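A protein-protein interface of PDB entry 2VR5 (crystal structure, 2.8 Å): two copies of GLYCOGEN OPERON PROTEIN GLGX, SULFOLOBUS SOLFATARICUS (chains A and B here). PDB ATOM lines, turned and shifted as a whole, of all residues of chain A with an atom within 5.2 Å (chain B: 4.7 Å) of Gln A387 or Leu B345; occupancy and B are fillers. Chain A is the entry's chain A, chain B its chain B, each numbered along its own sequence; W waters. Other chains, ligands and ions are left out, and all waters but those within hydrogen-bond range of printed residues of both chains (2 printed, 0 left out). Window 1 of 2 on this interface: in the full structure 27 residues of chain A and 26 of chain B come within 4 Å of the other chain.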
ATOM      1  N   ILE A 383      18.794  15.122  32.674  1.00  0.00           N
ATOM      2  CA  ILE A 383      19.668  14.145  32.036  1.00  0.00           C
ATOM      3  C   ILE A 383      18.928  12.841  31.761  1.00  0.00           C
ATOM      4  O   ILE A 383      19.052  12.261  30.681  1.00  0.00           O
ATOM      5  CB  ILE A 383      20.908  13.848  32.899  1.00  0.00           C
ATOM      6  CG1 ILE A 383      21.723  15.125  33.119  1.00  0.00           C
ATOM      7  CG2 ILE A 383      21.762  12.769  32.252  1.00  0.00           C
ATOM      8  CD1 ILE A 383      22.790  14.993  34.184  1.00  0.00           C
ATOM      9  N   ALA A 384      18.159  12.383  32.743  1.00  0.00           N
ATOM     10  CA  ALA A 384      17.275  11.238  32.556  1.00  0.00           C
ATOM     11  C   ALA A 384      16.291  11.483  31.417  1.00  0.00           C
ATOM     12  O   ALA A 384      16.051  10.601  30.591  1.00  0.00           O
ATOM     13  CB  ALA A 384      16.531  10.926  33.845  1.00  0.00           C
ATOM     14  N   LEU A 385      15.724  12.683  31.379  1.00  0.00           N
ATOM     15  CA  LEU A 385      14.795  13.059  30.319  1.00  0.00           C
ATOM     16  C   LEU A 385      15.478  13.041  28.956  1.00  0.00           C
ATOM     17  O   LEU A 385      14.831  12.830  27.930  1.00  0.00           O
ATOM     18  CB  LEU A 385      14.202  14.443  30.592  1.00  0.00           C
ATOM     19  CG  LEU A 385      13.191  14.961  29.568  1.00  0.00           C
ATOM     20  CD1 LEU A 385      13.898  15.683  28.432  1.00  0.00           C
ATOM     21  CD2 LEU A 385      12.335  13.822  29.033  1.00  0.00           C
ATOM     22  N   GLN A 386      16.788  13.264  28.952  1.00  0.00           N
ATOM     23  CA  GLN A 386      17.531  13.445  27.711  1.00  0.00           C
ATOM     24  C   GLN A 386      17.924  12.103  27.101  1.00  0.00           C
ATOM     25  O   GLN A 386      18.044  11.975  25.883  1.00  0.00           O
ATOM     26  CB  GLN A 386      18.778  14.298  27.952  1.00  0.00           C
ATOM     27  CG  GLN A 386      19.366  14.910  26.691  1.00  0.00           C
ATOM     28  CD  GLN A 386      20.728  15.531  26.926  1.00  0.00           C
ATOM     29  OE1 GLN A 386      21.732  14.828  27.043  1.00  0.00           O
ATOM     30  NE2 GLN A 386      20.771  16.856  26.993  1.00  0.00           N
ATOM     31  N   GLN A 387      18.123  11.107  27.958  1.00  0.00           N
ATOM     32  CA  GLN A 387      18.598   9.800  27.516  1.00  0.00           C
ATOM     33  C   GLN A 387      17.432   8.866  27.209  1.00  0.00           C
ATOM     34  O   GLN A 387      17.620   7.790  26.641  1.00  0.00           O
ATOM     35  CB  GLN A 387      19.508   9.175  28.574  1.00  0.00           C
ATOM     36  CG  GLN A 387      18.862   9.031  29.942  1.00  0.00           C
ATOM     37  CD  GLN A 387      17.975   7.806  30.041  1.00  0.00           C
ATOM     38  OE1 GLN A 387      18.426   6.680  29.833  1.00  0.00           O
ATOM     39  NE2 GLN A 387      16.704   8.020  30.362  1.00  0.00           N
ATOM     40  N   ASP A 388      16.229   9.284  27.587  1.00  0.00           N
ATOM     41  CA  ASP A 388      15.054   8.427  27.486  1.00  0.00           C
ATOM     42  C   ASP A 388      14.701   8.144  26.029  1.00  0.00           C
ATOM     43  O   ASP A 388      14.631   9.059  25.209  1.00  0.00           O
ATOM     44  CB  ASP A 388      13.861   9.067  28.201  1.00  0.00           C
ATOM     45  CG  ASP A 388      12.715   8.096  28.404  1.00  0.00           C
ATOM     46  OD1 ASP A 388      12.862   7.163  29.222  1.00  0.00           O
ATOM     47  OD2 ASP A 388      11.667   8.265  27.747  1.00  0.00           O
ATOM     48  N   PRO A 389      14.479   6.872  25.716  1.00  0.00           N
ATOM     49  CA  PRO A 389      14.233   6.451  24.334  1.00  0.00           C
ATOM     50  C   PRO A 389      12.925   7.020  23.793  1.00  0.00           C
ATOM     51  O   PRO A 389      12.875   7.466  22.646  1.00  0.00           O
ATOM     52  CB  PRO A 389      14.134   4.929  24.450  1.00  0.00           C
ATOM     53  CG  PRO A 389      14.972   4.592  25.631  1.00  0.00           C
ATOM     54  CD  PRO A 389      14.802   5.733  26.594  1.00  0.00           C
ATOM     55  N   SER A 392      13.044  11.191  24.062  1.00  0.00           N
ATOM     56  CA  SER A 392      14.070  11.760  23.195  1.00  0.00           C
ATOM     57  C   SER A 392      13.506  12.091  21.817  1.00  0.00           C
ATOM     58  O   SER A 392      14.206  12.639  20.965  1.00  0.00           O
ATOM     59  CB  SER A 392      15.253  10.798  23.062  1.00  0.00           C
ATOM     60  OG  SER A 392      14.950   9.737  22.173  1.00  0.00           O
ATOM     61  N   ILE B 341      26.509   8.558  30.802  1.00  0.00           N
ATOM     62  CA  ILE B 341      25.380   7.920  31.469  1.00  0.00           C
ATOM     63  C   ILE B 341      24.395   7.346  30.457  1.00  0.00           C
ATOM     64  O   ILE B 341      23.807   6.288  30.679  1.00  0.00           O
ATOM     65  CB  ILE B 341      24.638   8.905  32.391  1.00  0.00           C
ATOM     66  CG1 ILE B 341      25.572   9.408  33.495  1.00  0.00           C
ATOM     67  CG2 ILE B 341      23.404   8.249  32.989  1.00  0.00           C
ATOM     68  CD1 ILE B 341      24.972  10.504  34.349  1.00  0.00           C
ATOM     69  N   GLN B 342      24.218   8.052  29.344  1.00  0.00           N
ATOM     70  CA  GLN B 342      23.294   7.621  28.302  1.00  0.00           C
ATOM     71  C   GLN B 342      23.795   6.358  27.608  1.00  0.00           C
ATOM     72  O   GLN B 342      23.010   5.479  27.255  1.00  0.00           O
ATOM     73  CB  GLN B 342      23.085   8.737  27.277  1.00  0.00           C
ATOM     74  CG  GLN B 342      22.215   8.339  26.095  1.00  0.00           C
ATOM     75  CD  GLN B 342      22.027   9.470  25.104  1.00  0.00           C
ATOM     76  OE1 GLN B 342      21.436   9.287  24.040  1.00  0.00           O
ATOM     77  NE2 GLN B 342      22.529  10.650  25.449  1.00  0.00           N
ATOM     78  N   MET B 343      25.108   6.277  27.415  1.00  0.00           N
ATOM     79  CA  MET B 343      25.712   5.141  26.730  1.00  0.00           C
ATOM     80  C   MET B 343      25.569   3.863  27.550  1.00  0.00           C
ATOM     81  O   MET B 343      25.130   2.832  27.040  1.00  0.00           O
ATOM     82  CB  MET B 343      27.189   5.414  26.438  1.00  0.00           C
ATOM     83  CG  MET B 343      27.888   4.302  25.672  1.00  0.00           C
ATOM     84  SD  MET B 343      29.669   4.281  25.948  1.00  0.00           S
ATOM     85  CE  MET B 343      30.227   5.362  24.634  1.00  0.00           C
ATOM     86  N   VAL B 344      25.941   3.938  28.824  1.00  0.00           N
ATOM     87  CA  VAL B 344      25.784   2.812  29.736  1.00  0.00           C
ATOM     88  C   VAL B 344      24.336   2.336  29.780  1.00  0.00           C
ATOM     89  O   VAL B 344      24.066   1.135  29.769  1.00  0.00           O
ATOM     90  CB  VAL B 344      26.239   3.172  31.163  1.00  0.00           C
ATOM     91  CG1 VAL B 344      25.982   2.011  32.111  1.00  0.00           C
ATOM     92  CG2 VAL B 344      27.710   3.559  31.168  1.00  0.00           C
ATOM     93  N   LEU B 345      23.407   3.285  29.831  1.00  0.00           N
ATOM     94  CA  LEU B 345      21.987   2.964  29.914  1.00  0.00           C
ATOM     95  C   LEU B 345      21.456   2.456  28.579  1.00  0.00           C
ATOM     96  O   LEU B 345      20.694   1.491  28.529  1.00  0.00           O
ATOM     97  CB  LEU B 345      21.187   4.187  30.367  1.00  0.00           C
ATOM     98  CG  LEU B 345      21.176   4.471  31.870  1.00  0.00           C
ATOM     99  CD1 LEU B 345      20.436   5.766  32.167  1.00  0.00           C
ATOM    100  CD2 LEU B 345      20.558   3.310  32.632  1.00  0.00           C
ATOM    101  N   ASP B 346      21.864   3.112  27.498  1.00  0.00           N
ATOM    102  CA  ASP B 346      21.633   2.593  26.154  1.00  0.00           C
ATOM    103  C   ASP B 346      22.097   1.146  26.033  1.00  0.00           C
ATOM    104  O   ASP B 346      21.339   0.273  25.612  1.00  0.00           O
ATOM    105  CB  ASP B 346      22.344   3.463  25.115  1.00  0.00           C
ATOM    106  CG  ASP B 346      21.530   4.679  24.718  1.00  0.00           C
ATOM    107  OD1 ASP B 346      22.027   5.489  23.908  1.00  0.00           O
ATOM    108  OD2 ASP B 346      20.395   4.824  25.215  1.00  0.00           O
ATOM    109  N   SER B 347      23.350   0.899  26.406  1.00  0.00           N
ATOM    110  CA  SER B 347      23.914  -0.444  26.349  1.00  0.00           C
ATOM    111  C   SER B 347      23.031  -1.445  27.088  1.00  0.00           C
ATOM    112  O   SER B 347      22.638  -2.470  26.531  1.00  0.00           O
ATOM    113  CB  SER B 347      25.327  -0.456  26.936  1.00  0.00           C
ATOM    114  OG  SER B 347      25.868  -1.766  26.938  1.00  0.00           O
ATOM    115  N   LEU B 348      22.723  -1.140  28.344  1.00  0.00           N
ATOM    116  CA  LEU B 348      21.903  -2.022  29.168  1.00  0.00           C
ATOM    117  C   LEU B 348      20.582  -2.347  28.481  1.00  0.00           C
ATOM    118  O   LEU B 348      20.169  -3.505  28.423  1.00  0.00           O
ATOM    119  CB  LEU B 348      21.644  -1.389  30.536  1.00  0.00           C
ATOM    120  CG  LEU B 348      22.815  -1.398  31.520  1.00  0.00           C
ATOM    121  CD1 LEU B 348      22.481  -0.584  32.761  1.00  0.00           C
ATOM    122  CD2 LEU B 348      23.192  -2.823  31.895  1.00  0.00           C
ATOM    123  N   ARG B 349      19.922  -1.317  27.962  1.00  0.00           N
ATOM    124  CA  ARG B 349      18.650  -1.491  27.270  1.00  0.00           C
ATOM    125  C   ARG B 349      18.823  -2.307  25.995  1.00  0.00           C
ATOM    126  O   ARG B 349      17.914  -3.025  25.576  1.00  0.00           O
ATOM    127  CB  ARG B 349      18.025  -0.133  26.947  1.00  0.00           C
ATOM    128  CG  ARG B 349      17.358   0.544  28.133  1.00  0.00           C
ATOM    129  CD  ARG B 349      16.507   1.723  27.689  1.00  0.00           C
ATOM    130  NE  ARG B 349      17.323   2.854  27.259  1.00  0.00           N
ATOM    131  CZ  ARG B 349      17.768   3.806  28.073  1.00  0.00           C
ATOM    132  NH1 ARG B 349      17.477   3.766  29.366  1.00  0.00           N
ATOM    133  NH2 ARG B 349      18.504   4.800  27.594  1.00  0.00           N
ATOM    134  N   PHE B 381      22.979   8.278  37.496  1.00  0.00           N
ATOM    135  CA  PHE B 381      22.928   7.034  36.737  1.00  0.00           C
ATOM    136  C   PHE B 381      21.961   6.041  37.372  1.00  0.00           C
ATOM    137  O   PHE B 381      21.055   5.534  36.711  1.00  0.00           O
ATOM    138  CB  PHE B 381      24.323   6.415  36.631  1.00  0.00           C
ATOM    139  CG  PHE B 381      24.317   4.982  36.178  1.00  0.00           C
ATOM    140  CD1 PHE B 381      25.027   4.018  36.876  1.00  0.00           C
ATOM    141  CD2 PHE B 381      23.602   4.599  35.057  1.00  0.00           C
ATOM    142  CE1 PHE B 381      25.023   2.700  36.462  1.00  0.00           C
ATOM    143  CE2 PHE B 381      23.595   3.282  34.638  1.00  0.00           C
ATOM    144  CZ  PHE B 381      24.306   2.331  35.342  1.00  0.00           C
ATOM    145  N   ALA B 384      18.181   7.347  37.086  1.00  0.00           N
ATOM    146  CA  ALA B 384      17.675   7.091  35.743  1.00  0.00           C
ATOM    147  C   ALA B 384      17.427   5.602  35.522  1.00  0.00           C
ATOM    148  O   ALA B 384      16.430   5.213  34.912  1.00  0.00           O
ATOM    149  CB  ALA B 384      18.641   7.629  34.700  1.00  0.00           C
ATOM    150  N   LEU B 385      18.338   4.774  36.023  1.00  0.00           N
ATOM    151  CA  LEU B 385      18.235   3.329  35.857  1.00  0.00           C
ATOM    152  C   LEU B 385      17.018   2.776  36.591  1.00  0.00           C
ATOM    153  O   LEU B 385      16.342   1.873  36.099  1.00  0.00           O
ATOM    154  CB  LEU B 385      19.507   2.641  36.353  1.00  0.00           C
ATOM    155  CG  LEU B 385      19.447   1.118  36.483  1.00  0.00           C
ATOM    156  CD1 LEU B 385      19.022   0.483  35.167  1.00  0.00           C
ATOM    157  CD2 LEU B 385      20.787   0.564  36.942  1.00  0.00           C
ATOM    158  N   GLN B 387      14.217   4.368  37.232  1.00  0.00           N
ATOM    159  CA  GLN B 387      12.955   4.884  36.717  1.00  0.00           C
ATOM    160  C   GLN B 387      12.687   4.377  35.305  1.00  0.00           C
ATOM    161  O   GLN B 387      11.621   4.619  34.738  1.00  0.00           O
ATOM    162  CB  GLN B 387      12.953   6.414  36.735  1.00  0.00           C
ATOM    163  CG  GLN B 387      14.025   7.045  35.862  1.00  0.00           C
ATOM    164  CD  GLN B 387      13.629   7.095  34.398  1.00  0.00           C
ATOM    165  OE1 GLN B 387      12.552   7.577  34.052  1.00  0.00           O
ATOM    166  NE2 GLN B 387      14.503   6.595  33.532  1.00  0.00           N
ATOM    167  N   LEU B 391      14.512  -1.438  31.986  1.00  0.00           N
ATOM    168  CA  LEU B 391      15.433  -1.996  32.969  1.00  0.00           C
ATOM    169  C   LEU B 391      14.754  -2.173  34.323  1.00  0.00           C
ATOM    170  O   LEU B 391      15.349  -2.702  35.262  1.00  0.00           O
ATOM    171  CB  LEU B 391      16.667  -1.104  33.113  1.00  0.00           C
ATOM    172  CG  LEU B 391      17.344  -0.667  31.812  1.00  0.00           C
ATOM    173  CD1 LEU B 391      18.491   0.290  32.098  1.00  0.00           C
ATOM    174  CD2 LEU B 391      17.831  -1.876  31.027  1.00  0.00           C
HETATM  175  O   HOH W   1      21.808  12.090  28.548  1.00  0.00           O
HETATM  176  O   HOH W   2      14.514   6.090  30.796  1.00  0.00           O
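Water W2 lies within hydrogen-bond range of the side-chain carboxylate (OD1) of Asp A388, the side-chain amide nitrogen (NE2) of Gln B387 and the side-chain amide nitrogen (NE2) of Gln A387. Water W1 lies within hydrogen-bond range of OE1 of Gln A386 (3.1 Å), O of Ile A383 (3.5 Å) and NE2 of Gln B342 (3.5 Å).
O of Ala A384 is in hydrogen-bond range of NE2 of Gln A387, 2.7 Å away. O of Pro A389 is in hydrogen-bond range of OG of Ser A392, 3.1 Å away. The side-chain carboxylate (OD2) of Asp B346 is in salt-bridge range of the guanidinium group (NH2) of Arg B349 (3.0 Å).
3 positions are printed for both chains. Of the 4 pairs that touch across the chains among the printed residues, none has its exchanged pair printed and touching as well.
Gln A387 touches Gln B342. Gln A387 touches Leu B345. NE of Arg B349 touches CG of Pro A389, 3.3 Å away.
Ile A383 touches none of the printed residues of chain B. Gln A387 touches three residues of chain B. Of the printed residues of chain B, Pro A389 touches Arg B349. Of the printed residues of chain A, Gln B342 touches Gln A387. Leu B345 touches just one residue of chain A: Gln A387. Of the printed residues of chain A, Arg B349 touches Gln A387 and Pro A389.
Hydrophobic or aromatic side chains of chain A within 4 Å of the printed part of chain B: Pro A389. Of the 14 printed residues of chain B, 3 touch a printed residue of chain A. Hydrophobic or aromatic side chains of chain B within 4 Å of the printed part of chain A: Leu B345. Among the printed residues, 4 pairs touch across the chains.
OE1 of Gln A387 lies within hydrogen-bond range of NH2 of Arg B349, 2.9 Å away.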
